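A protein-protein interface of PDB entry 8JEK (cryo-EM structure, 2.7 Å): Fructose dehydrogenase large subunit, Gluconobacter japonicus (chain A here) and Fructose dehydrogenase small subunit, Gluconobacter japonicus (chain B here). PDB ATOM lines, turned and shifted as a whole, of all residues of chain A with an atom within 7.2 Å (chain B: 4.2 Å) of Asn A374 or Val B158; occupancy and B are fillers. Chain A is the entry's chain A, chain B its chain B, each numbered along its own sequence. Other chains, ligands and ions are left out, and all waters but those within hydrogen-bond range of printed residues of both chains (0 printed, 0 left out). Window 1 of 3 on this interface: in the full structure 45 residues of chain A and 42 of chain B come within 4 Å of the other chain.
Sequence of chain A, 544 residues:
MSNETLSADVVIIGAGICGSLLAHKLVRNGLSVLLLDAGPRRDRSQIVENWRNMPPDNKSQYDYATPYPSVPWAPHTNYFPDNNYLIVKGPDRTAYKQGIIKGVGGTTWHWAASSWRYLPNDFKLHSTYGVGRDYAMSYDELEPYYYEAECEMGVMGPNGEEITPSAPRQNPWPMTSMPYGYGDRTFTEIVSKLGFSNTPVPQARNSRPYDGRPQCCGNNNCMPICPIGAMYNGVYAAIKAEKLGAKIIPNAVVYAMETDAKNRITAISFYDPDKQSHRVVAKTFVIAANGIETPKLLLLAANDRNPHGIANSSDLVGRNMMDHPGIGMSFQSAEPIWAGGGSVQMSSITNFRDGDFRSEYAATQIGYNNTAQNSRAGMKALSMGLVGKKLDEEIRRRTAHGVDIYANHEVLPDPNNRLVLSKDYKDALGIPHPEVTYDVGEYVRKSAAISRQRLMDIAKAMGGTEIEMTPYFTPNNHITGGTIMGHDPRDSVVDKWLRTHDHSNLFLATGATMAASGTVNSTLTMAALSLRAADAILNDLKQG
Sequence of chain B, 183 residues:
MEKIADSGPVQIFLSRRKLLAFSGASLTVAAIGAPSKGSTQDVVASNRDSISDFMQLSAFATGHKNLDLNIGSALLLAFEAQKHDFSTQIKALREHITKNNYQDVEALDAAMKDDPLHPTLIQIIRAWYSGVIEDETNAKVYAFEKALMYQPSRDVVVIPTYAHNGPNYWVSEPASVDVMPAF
O of Cys A217 touches CE1 of Tyr B169 (3.8 Å).
Gly A218 touches Val B158.
CB of Asn A220 touches CG1 of Val B158, at 3.8 Å.
Val B157 touches Ala A339.
Gly A340 touches Val B158 (O to CG1, 3.5 Å).
OH of Tyr B169 touches O of Gly A340 (3.7 Å).
CB of Ala A372 touches CG1 of Val B157 (3.7 Å).
CB of Ala A372 touches O of Val B158, 3.9 Å away.
Asn A374 touches Tyr B150.
Val B157 touches Thr A399 (CG2 to CG2, 3.7 Å).
O of Pro B160 is in hydrogen-bond range of ND2 of Asn A219 (3.1 Å).
ND2 of Asn A219 lies close to O of Tyr B162, 3.4 Å away.
The side-chain amide nitrogen (ND2) of Asn A374 sits at hydrogen-bond distance from the backbone carbonyl oxygen (O) of Val B158 (2.8 Å).
The side-chain hydroxyl (OH) of Tyr B150 sits at hydrogen-bond distance from the side-chain hydroxyl (OG) of Ser A375 (2.6 Å).
Hydrophobic or aromatic side chains of chain B that line the printed part of chain A: Tyr B150, Val B157, Val B158, Pro B160 and Tyr B169.
Along chain A the printed residues that touch a printed residue of chain B span positions 217 to 399.
Printed residues of chain B within 4 Å of Asn A220: Val B158 (3.8 Å).
Of the printed residues of chain B, Gly A340 touches Val B158 (3.5 Å) and Tyr B169 (3.7 Å).
Of chain B, only Tyr B150 (3.7 Å) and Val B158 (2.8 Å) come within 4 Å of Asn A374.
Of the printed residues of chain B, Thr A399 touches Val B157 (3.7 Å).
The nearest printed residue of chain B that does not touch Asn A374 is Val B157 (4.1 Å).
The side-chain sulfur of Cys A217 sits at hydrogen-bond distance from the side-chain amide oxygen of Asn A219.
The side-chain amide nitrogen of Asn A220 lies within hydrogen-bond range of the backbone carbonyl oxygen of Asn A370, 3.1 Å away.
The backbone NH of Ala A372 lies close to the side-chain amide nitrogen of Asn A220 (2.9 Å).
N of Gly A340 lies within hydrogen-bond range of O of Asn A370 (3.3 Å).
The side-chain hydroxyl (OG1) of Thr A399 is in hydrogen-bond range of the backbone carbonyl oxygen (O) of Ile A395, at 2.5 Å.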
ATOM      1  N   SER A  60      24.117   5.526 -19.318  1.00  0.00           N
ATOM      2  CA  SER A  60      24.317   5.111 -17.934  1.00  0.00           C
ATOM      3  C   SER A  60      24.984   3.745 -17.866  1.00  0.00           C
ATOM      4  O   SER A  60      26.004   3.570 -17.191  1.00  0.00           O
ATOM      5  CB  SER A  60      22.976   5.095 -17.201  1.00  0.00           C
ATOM      6  OG  SER A  60      23.038   4.296 -16.036  1.00  0.00           O
ATOM      7  N   CYS A 217      40.774  18.091 -23.339  1.00  0.00           N
ATOM      8  CA  CYS A 217      39.997  19.006 -22.514  1.00  0.00           C
ATOM      9  C   CYS A 217      39.098  18.284 -21.522  1.00  0.00           C
ATOM     10  O   CYS A 217      38.210  18.913 -20.941  1.00  0.00           O
ATOM     11  CB  CYS A 217      39.158  19.937 -23.391  1.00  0.00           C
ATOM     12  SG  CYS A 217      37.958  19.125 -24.459  1.00  0.00           S
ATOM     13  N   GLY A 218      39.311  16.991 -21.311  1.00  0.00           N
ATOM     14  CA  GLY A 218      38.488  16.230 -20.391  1.00  0.00           C
ATOM     15  C   GLY A 218      37.056  16.037 -20.832  1.00  0.00           C
ATOM     16  O   GLY A 218      36.139  16.183 -20.016  1.00  0.00           O
ATOM     17  N   ASN A 219      36.838  15.715 -22.109  1.00  0.00           N
ATOM     18  CA  ASN A 219      35.495  15.402 -22.581  1.00  0.00           C
ATOM     19  C   ASN A 219      34.944  14.128 -21.954  1.00  0.00           C
ATOM     20  O   ASN A 219      33.734  13.908 -22.002  1.00  0.00           O
ATOM     21  CB  ASN A 219      35.479  15.278 -24.103  1.00  0.00           C
ATOM     22  CG  ASN A 219      35.281  16.610 -24.795  1.00  0.00           C
ATOM     23  OD1 ASN A 219      36.005  16.953 -25.726  1.00  0.00           O
ATOM     24  ND2 ASN A 219      34.297  17.367 -24.343  1.00  0.00           N
ATOM     25  N   ASN A 220      35.799  13.281 -21.385  1.00  0.00           N
ATOM     26  CA  ASN A 220      35.359  12.134 -20.592  1.00  0.00           C
ATOM     27  C   ASN A 220      34.472  11.184 -21.391  1.00  0.00           C
ATOM     28  O   ASN A 220      33.581  10.537 -20.837  1.00  0.00           O
ATOM     29  CB  ASN A 220      34.632  12.591 -19.327  1.00  0.00           C
ATOM     30  CG  ASN A 220      34.786  11.619 -18.189  1.00  0.00           C
ATOM     31  OD1 ASN A 220      35.761  10.881 -18.115  1.00  0.00           O
ATOM     32  ND2 ASN A 220      33.805  11.593 -17.307  1.00  0.00           N
ATOM     33  N   ASN A 221      34.693  11.098 -22.696  1.00  0.00           N
ATOM     34  CA  ASN A 221      33.948  10.198 -23.565  1.00  0.00           C
ATOM     35  C   ASN A 221      34.901   9.356 -24.392  1.00  0.00           C
ATOM     36  O   ASN A 221      34.627   9.030 -25.549  1.00  0.00           O
ATOM     37  CB  ASN A 221      32.993  10.972 -24.469  1.00  0.00           C
ATOM     38  CG  ASN A 221      31.784  10.159 -24.865  1.00  0.00           C
ATOM     39  OD1 ASN A 221      31.162   9.510 -24.031  1.00  0.00           O
ATOM     40  ND2 ASN A 221      31.450  10.180 -26.147  1.00  0.00           N
ATOM     41  N   ALA A 339      33.153  12.003  -9.957  1.00  0.00           N
ATOM     42  CA  ALA A 339      33.725  11.378 -11.141  1.00  0.00           C
ATOM     43  C   ALA A 339      33.424  12.213 -12.378  1.00  0.00           C
ATOM     44  O   ALA A 339      32.319  12.734 -12.540  1.00  0.00           O
ATOM     45  CB  ALA A 339      33.174   9.963 -11.314  1.00  0.00           C
ATOM     46  N   GLY A 340      34.418  12.344 -13.254  1.00  0.00           N
ATOM     47  CA  GLY A 340      34.213  13.059 -14.497  1.00  0.00           C
ATOM     48  C   GLY A 340      35.336  13.989 -14.909  1.00  0.00           C
ATOM     49  O   GLY A 340      35.329  14.510 -16.027  1.00  0.00           O
ATOM     50  N   GLY A 341      36.307  14.207 -14.026  1.00  0.00           N
ATOM     51  CA  GLY A 341      37.386  15.132 -14.311  1.00  0.00           C
ATOM     52  C   GLY A 341      38.580  14.492 -14.987  1.00  0.00           C
ATOM     53  O   GLY A 341      39.405  13.851 -14.330  1.00  0.00           O
ATOM     54  N   GLY A 342      38.690  14.665 -16.300  1.00  0.00           N
ATOM     55  CA  GLY A 342      39.790  14.089 -17.047  1.00  0.00           C
ATOM     56  C   GLY A 342      39.318  13.093 -18.081  1.00  0.00           C
ATOM     57  O   GLY A 342      38.297  13.311 -18.738  1.00  0.00           O
ATOM     58  N   ASN A 370      36.461   6.563 -14.148  1.00  0.00           N
ATOM     59  CA  ASN A 370      36.377   8.013 -14.064  1.00  0.00           C
ATOM     60  C   ASN A 370      35.274   8.585 -14.948  1.00  0.00           C
ATOM     61  O   ASN A 370      35.207   9.803 -15.137  1.00  0.00           O
ATOM     62  CB  ASN A 370      37.732   8.624 -14.423  1.00  0.00           C
ATOM     63  CG  ASN A 370      37.871  10.060 -13.970  1.00  0.00           C
ATOM     64  OD1 ASN A 370      37.448  10.422 -12.875  1.00  0.00           O
ATOM     65  ND2 ASN A 370      38.467  10.886 -14.815  1.00  0.00           N
ATOM     66  N   THR A 371      34.413   7.736 -15.501  1.00  0.00           N
ATOM     67  CA  THR A 371      33.306   8.222 -16.309  1.00  0.00           C
ATOM     68  C   THR A 371      32.303   8.968 -15.437  1.00  0.00           C
ATOM     69  O   THR A 371      32.056   8.592 -14.289  1.00  0.00           O
ATOM     70  CB  THR A 371      32.615   7.065 -17.029  1.00  0.00           C
ATOM     71  OG1 THR A 371      33.593   6.097 -17.426  1.00  0.00           O
ATOM     72  CG2 THR A 371      31.887   7.567 -18.261  1.00  0.00           C
ATOM     73  N   ALA A 372      31.732  10.035 -15.990  1.00  0.00           N
ATOM     74  CA  ALA A 372      30.794  10.857 -15.240  1.00  0.00           C
ATOM     75  C   ALA A 372      29.552  10.058 -14.873  1.00  0.00           C
ATOM     76  O   ALA A 372      29.053   9.251 -15.663  1.00  0.00           O
ATOM     77  CB  ALA A 372      30.407  12.091 -16.055  1.00  0.00           C
ATOM     78  N   GLN A 373      29.050  10.287 -13.662  1.00  0.00           N
ATOM     79  CA  GLN A 373      27.901   9.563 -13.140  1.00  0.00           C
ATOM     80  C   GLN A 373      26.605  10.353 -13.261  1.00  0.00           C
ATOM     81  O   GLN A 373      25.621  10.014 -12.598  1.00  0.00           O
ATOM     82  CB  GLN A 373      28.140   9.172 -11.681  1.00  0.00           C
ATOM     83  CG  GLN A 373      29.299   8.216 -11.472  1.00  0.00           C
ATOM     84  CD  GLN A 373      28.903   6.768 -11.653  1.00  0.00           C
ATOM     85  OE1 GLN A 373      27.860   6.333 -11.174  1.00  0.00           O
ATOM     86  NE2 GLN A 373      29.740   6.011 -12.348  1.00  0.00           N
ATOM     87  N   ASN A 374      26.580  11.398 -14.091  1.00  0.00           N
ATOM     88  CA  ASN A 374      25.386  12.232 -14.182  1.00  0.00           C
ATOM     89  C   ASN A 374      24.236  11.512 -14.872  1.00  0.00           C
ATOM     90  O   ASN A 374      23.082  11.649 -14.449  1.00  0.00           O
ATOM     91  CB  ASN A 374      25.709  13.544 -14.898  1.00  0.00           C
ATOM     92  CG  ASN A 374      26.614  13.354 -16.094  1.00  0.00           C
ATOM     93  OD1 ASN A 374      26.880  12.231 -16.516  1.00  0.00           O
ATOM     94  ND2 ASN A 374      27.097  14.457 -16.648  1.00  0.00           N
ATOM     95  N   SER A 375      24.519  10.739 -15.922  1.00  0.00           N
ATOM     96  CA  SER A 375      23.467   9.971 -16.580  1.00  0.00           C
ATOM     97  C   SER A 375      22.900   8.896 -15.661  1.00  0.00           C
ATOM     98  O   SER A 375      21.677   8.758 -15.541  1.00  0.00           O
ATOM     99  CB  SER A 375      24.002   9.338 -17.864  1.00  0.00           C
ATOM    100  OG  SER A 375      23.910  10.236 -18.953  1.00  0.00           O
ATOM    101  N   ARG A 376      23.777   8.134 -15.001  1.00  0.00           N
ATOM    102  CA  ARG A 376      23.320   7.102 -14.077  1.00  0.00           C
ATOM    103  C   ARG A 376      22.556   7.704 -12.908  1.00  0.00           C
ATOM    104  O   ARG A 376      21.516   7.173 -12.502  1.00  0.00           O
ATOM    105  CB  ARG A 376      24.507   6.287 -13.568  1.00  0.00           C
ATOM    106  CG  ARG A 376      24.101   5.048 -12.793  1.00  0.00           C
ATOM    107  CD  ARG A 376      25.248   4.073 -12.669  1.00  0.00           C
ATOM    108  NE  ARG A 376      25.664   3.557 -13.966  1.00  0.00           N
ATOM    109  CZ  ARG A 376      26.847   3.011 -14.206  1.00  0.00           C
ATOM    110  NH1 ARG A 376      27.758   2.891 -13.256  1.00  0.00           N
ATOM    111  NH2 ARG A 376      27.122   2.574 -15.431  1.00  0.00           N
ATOM    112  N   ALA A 377      23.060   8.807 -12.348  1.00  0.00           N
ATOM    113  CA  ALA A 377      22.376   9.453 -11.235  1.00  0.00           C
ATOM    114  C   ALA A 377      21.005   9.965 -11.649  1.00  0.00           C
ATOM    115  O   ALA A 377      20.026   9.793 -10.915  1.00  0.00           O
ATOM    116  CB  ALA A 377      23.226  10.593 -10.688  1.00  0.00           C
ATOM    117  N   GLY A 378      20.915  10.593 -12.824  1.00  0.00           N
ATOM    118  CA  GLY A 378      19.625  11.068 -13.293  1.00  0.00           C
ATOM    119  C   GLY A 378      18.639   9.940 -13.510  1.00  0.00           C
ATOM    120  O   GLY A 378      17.479  10.025 -13.099  1.00  0.00           O
ATOM    121  N   MET A 379      19.091   8.856 -14.145  1.00  0.00           N
ATOM    122  CA  MET A 379      18.210   7.719 -14.388  1.00  0.00           C
ATOM    123  C   MET A 379      17.731   7.105 -13.078  1.00  0.00           C
ATOM    124  O   MET A 379      16.539   6.812 -12.913  1.00  0.00           O
ATOM    125  CB  MET A 379      18.932   6.673 -15.238  1.00  0.00           C
ATOM    126  CG  MET A 379      19.128   7.070 -16.687  1.00  0.00           C
ATOM    127  SD  MET A 379      17.617   6.945 -17.654  1.00  0.00           S
ATOM    128  CE  MET A 379      17.163   8.665 -17.771  1.00  0.00           C
ATOM    129  N   LYS A 380      18.648   6.913 -12.126  1.00  0.00           N
ATOM    130  CA  LYS A 380      18.276   6.309 -10.853  1.00  0.00           C
ATOM    131  C   LYS A 380      17.312   7.196 -10.079  1.00  0.00           C
ATOM    132  O   LYS A 380      16.340   6.704  -9.496  1.00  0.00           O
ATOM    133  CB  LYS A 380      19.524   6.021 -10.023  1.00  0.00           C
ATOM    134  CG  LYS A 380      19.232   5.351  -8.693  1.00  0.00           C
ATOM    135  CD  LYS A 380      18.778   3.916  -8.888  1.00  0.00           C
ATOM    136  CE  LYS A 380      18.688   3.182  -7.565  1.00  0.00           C
ATOM    137  NZ  LYS A 380      17.592   3.708  -6.713  1.00  0.00           N
ATOM    138  N   ILE A 395      19.675  13.745  -7.656  1.00  0.00           N
ATOM    139  CA  ILE A 395      20.545  13.692  -8.829  1.00  0.00           C
ATOM    140  C   ILE A 395      21.935  14.206  -8.483  1.00  0.00           C
ATOM    141  O   ILE A 395      22.946  13.577  -8.822  1.00  0.00           O
ATOM    142  CB  ILE A 395      19.932  14.481 -10.001  1.00  0.00           C
ATOM    143  CG1 ILE A 395      18.612  13.854 -10.446  1.00  0.00           C
ATOM    144  CG2 ILE A 395      20.906  14.540 -11.165  1.00  0.00           C
ATOM    145  CD1 ILE A 395      17.876  14.658 -11.489  1.00  0.00           C
ATOM    146  N   ARG A 398      23.788  11.690  -6.057  1.00  0.00           N
ATOM    147  CA  ARG A 398      24.225  10.458  -6.697  1.00  0.00           C
ATOM    148  C   ARG A 398      25.274  10.711  -7.772  1.00  0.00           C
ATOM    149  O   ARG A 398      26.083   9.823  -8.057  1.00  0.00           O
ATOM    150  CB  ARG A 398      23.023   9.716  -7.282  1.00  0.00           C
ATOM    151  CG  ARG A 398      21.951   9.392  -6.262  1.00  0.00           C
ATOM    152  CD  ARG A 398      20.853   8.537  -6.859  1.00  0.00           C
ATOM    153  NE  ARG A 398      21.099   7.119  -6.637  1.00  0.00           N
ATOM    154  CZ  ARG A 398      20.887   6.491  -5.489  1.00  0.00           C
ATOM    155  NH1 ARG A 398      20.408   7.125  -4.432  1.00  0.00           N
ATOM    156  NH2 ARG A 398      21.160   5.193  -5.400  1.00  0.00           N
ATOM    157  N   THR A 399      25.277  11.899  -8.380  1.00  0.00           N
ATOM    158  CA  THR A 399      26.374  12.277  -9.260  1.00  0.00           C
ATOM    159  C   THR A 399      27.665  12.512  -8.494  1.00  0.00           C
ATOM    160  O   THR A 399      28.743  12.180  -8.999  1.00  0.00           O
ATOM    161  CB  THR A 399      26.012  13.537 -10.047  1.00  0.00           C
ATOM    162  OG1 THR A 399      24.678  13.424 -10.552  1.00  0.00           O
ATOM    163  CG2 THR A 399      26.966  13.730 -11.210  1.00  0.00           C
ATOM    164  N   ALA A 400      27.576  13.072  -7.287  1.00  0.00           N
ATOM    165  CA  ALA A 400      28.761  13.319  -6.479  1.00  0.00           C
ATOM    166  C   ALA A 400      29.290  12.060  -5.804  1.00  0.00           C
ATOM    167  O   ALA A 400      30.487  11.983  -5.512  1.00  0.00           O
ATOM    168  CB  ALA A 400      28.456  14.375  -5.419  1.00  0.00           C
ATOM    169  N   TYR B 150      21.172  16.773 -16.137  1.00  0.00           N
ATOM    170  CA  TYR B 150      22.566  17.176 -16.240  1.00  0.00           C
ATOM    171  C   TYR B 150      22.831  18.535 -15.616  1.00  0.00           C
ATOM    172  O   TYR B 150      23.994  18.930 -15.496  1.00  0.00           O
ATOM    173  CB  TYR B 150      22.997  17.199 -17.708  1.00  0.00           C
ATOM    174  CG  TYR B 150      22.915  15.854 -18.384  1.00  0.00           C
ATOM    175  CD1 TYR B 150      23.680  14.788 -17.943  1.00  0.00           C
ATOM    176  CD2 TYR B 150      22.070  15.651 -19.465  1.00  0.00           C
ATOM    177  CE1 TYR B 150      23.608  13.560 -18.555  1.00  0.00           C
ATOM    178  CE2 TYR B 150      21.991  14.423 -20.083  1.00  0.00           C
ATOM    179  CZ  TYR B 150      22.764  13.381 -19.624  1.00  0.00           C
ATOM    180  OH  TYR B 150      22.691  12.154 -20.237  1.00  0.00           O
ATOM    181  N   VAL B 156      30.025  21.293 -11.811  1.00  0.00           N
ATOM    182  CA  VAL B 156      31.195  20.500 -11.455  1.00  0.00           C
ATOM    183  C   VAL B 156      31.460  19.407 -12.482  1.00  0.00           C
ATOM    184  O   VAL B 156      32.588  19.245 -12.955  1.00  0.00           O
ATOM    185  CB  VAL B 156      31.052  19.892 -10.042  1.00  0.00           C
ATOM    186  CG1 VAL B 156      32.275  19.069  -9.699  1.00  0.00           C
ATOM    187  CG2 VAL B 156      30.834  20.982  -9.011  1.00  0.00           C
ATOM    188  N   VAL B 157      30.429  18.651 -12.845  1.00  0.00           N
ATOM    189  CA  VAL B 157      30.576  17.453 -13.665  1.00  0.00           C
ATOM    190  C   VAL B 157      30.364  17.809 -15.127  1.00  0.00           C
ATOM    191  O   VAL B 157      29.515  18.642 -15.467  1.00  0.00           O
ATOM    192  CB  VAL B 157      29.599  16.350 -13.218  1.00  0.00           C
ATOM    193  CG1 VAL B 157      30.001  15.014 -13.817  1.00  0.00           C
ATOM    194  CG2 VAL B 157      29.566  16.265 -11.710  1.00  0.00           C
ATOM    195  N   VAL B 158      31.141  17.165 -15.996  1.00  0.00           N
ATOM    196  CA  VAL B 158      31.070  17.426 -17.426  1.00  0.00           C
ATOM    197  C   VAL B 158      29.871  16.705 -18.029  1.00  0.00           C
ATOM    198  O   VAL B 158      29.499  15.605 -17.600  1.00  0.00           O
ATOM    199  CB  VAL B 158      32.385  16.993 -18.099  1.00  0.00           C
ATOM    200  CG1 VAL B 158      32.581  15.490 -17.990  1.00  0.00           C
ATOM    201  CG2 VAL B 158      32.423  17.424 -19.544  1.00  0.00           C
ATOM    202  N   ILE B 159      29.236  17.341 -19.009  1.00  0.00           N
ATOM    203  CA  ILE B 159      28.320  16.642 -19.904  1.00  0.00           C
ATOM    204  C   ILE B 159      29.190  16.135 -21.047  1.00  0.00           C
ATOM    205  O   ILE B 159      29.632  16.932 -21.886  1.00  0.00           O
ATOM    206  CB  ILE B 159      27.179  17.553 -20.381  1.00  0.00           C
ATOM    207  CG1 ILE B 159      26.440  18.141 -19.178  1.00  0.00           C
ATOM    208  CG2 ILE B 159      26.213  16.785 -21.259  1.00  0.00           C
ATOM    209  CD1 ILE B 159      25.439  19.200 -19.535  1.00  0.00           C
ATOM    210  N   PRO B 160      29.445  14.821 -21.120  1.00  0.00           N
ATOM    211  CA  PRO B 160      30.659  14.312 -21.777  1.00  0.00           C
ATOM    212  C   PRO B 160      31.061  14.918 -23.116  1.00  0.00           C
ATOM    213  O   PRO B 160      32.147  15.493 -23.214  1.00  0.00           O
ATOM    214  CB  PRO B 160      30.339  12.824 -21.923  1.00  0.00           C
ATOM    215  CG  PRO B 160      29.599  12.529 -20.667  1.00  0.00           C
ATOM    216  CD  PRO B 160      28.729  13.743 -20.415  1.00  0.00           C
ATOM    217  N   TYR B 162      30.671  17.568 -24.483  1.00  0.00           N
ATOM    218  CA  TYR B 162      30.888  19.004 -24.458  1.00  0.00           C
ATOM    219  C   TYR B 162      31.882  19.326 -23.352  1.00  0.00           C
ATOM    220  O   TYR B 162      31.920  18.653 -22.321  1.00  0.00           O
ATOM    221  CB  TYR B 162      29.578  19.762 -24.242  1.00  0.00           C
ATOM    222  CG  TYR B 162      28.555  19.497 -25.320  1.00  0.00           C
ATOM    223  CD1 TYR B 162      27.675  18.428 -25.223  1.00  0.00           C
ATOM    224  CD2 TYR B 162      28.479  20.307 -26.444  1.00  0.00           C
ATOM    225  CE1 TYR B 162      26.746  18.181 -26.207  1.00  0.00           C
ATOM    226  CE2 TYR B 162      27.554  20.065 -27.433  1.00  0.00           C
ATOM    227  CZ  TYR B 162      26.689  19.002 -27.311  1.00  0.00           C
ATOM    228  OH  TYR B 162      25.763  18.759 -28.298  1.00  0.00           O
ATOM    229  N   HIS B 164      33.980  21.293 -20.418  1.00  0.00           N
ATOM    230  CA  HIS B 164      34.155  22.292 -19.376  1.00  0.00           C
ATOM    231  C   HIS B 164      35.300  23.232 -19.756  1.00  0.00           C
ATOM    232  O   HIS B 164      36.015  23.024 -20.741  1.00  0.00           O
ATOM    233  CB  HIS B 164      34.441  21.616 -18.037  1.00  0.00           C
ATOM    234  CG  HIS B 164      33.342  21.746 -17.030  1.00  0.00           C
ATOM    235  ND1 HIS B 164      33.411  22.616 -15.964  1.00  0.00           N
ATOM    236  CD2 HIS B 164      32.155  21.107 -16.917  1.00  0.00           C
ATOM    237  CE1 HIS B 164      32.312  22.510 -15.239  1.00  0.00           C
ATOM    238  NE2 HIS B 164      31.533  21.603 -15.798  1.00  0.00           N
ATOM    239  N   TYR B 169      40.945  21.951 -16.350  1.00  0.00           N
ATOM    240  CA  TYR B 169      40.086  22.607 -15.371  1.00  0.00           C
ATOM    241  C   TYR B 169      39.938  21.815 -14.080  1.00  0.00           C
ATOM    242  O   TYR B 169      39.543  22.389 -13.060  1.00  0.00           O
ATOM    243  CB  TYR B 169      38.705  22.859 -15.979  1.00  0.00           C
ATOM    244  CG  TYR B 169      37.854  21.615 -16.110  1.00  0.00           C
ATOM    245  CD1 TYR B 169      37.939  20.809 -17.236  1.00  0.00           C
ATOM    246  CD2 TYR B 169      36.963  21.248 -15.110  1.00  0.00           C
ATOM    247  CE1 TYR B 169      37.170  19.673 -17.356  1.00  0.00           C
ATOM    248  CE2 TYR B 169      36.193  20.113 -15.222  1.00  0.00           C
ATOM    249  CZ  TYR B 169      36.299  19.330 -16.347  1.00  0.00           C
ATOM    250  OH  TYR B 169      35.527  18.198 -16.464  1.00  0.00           O
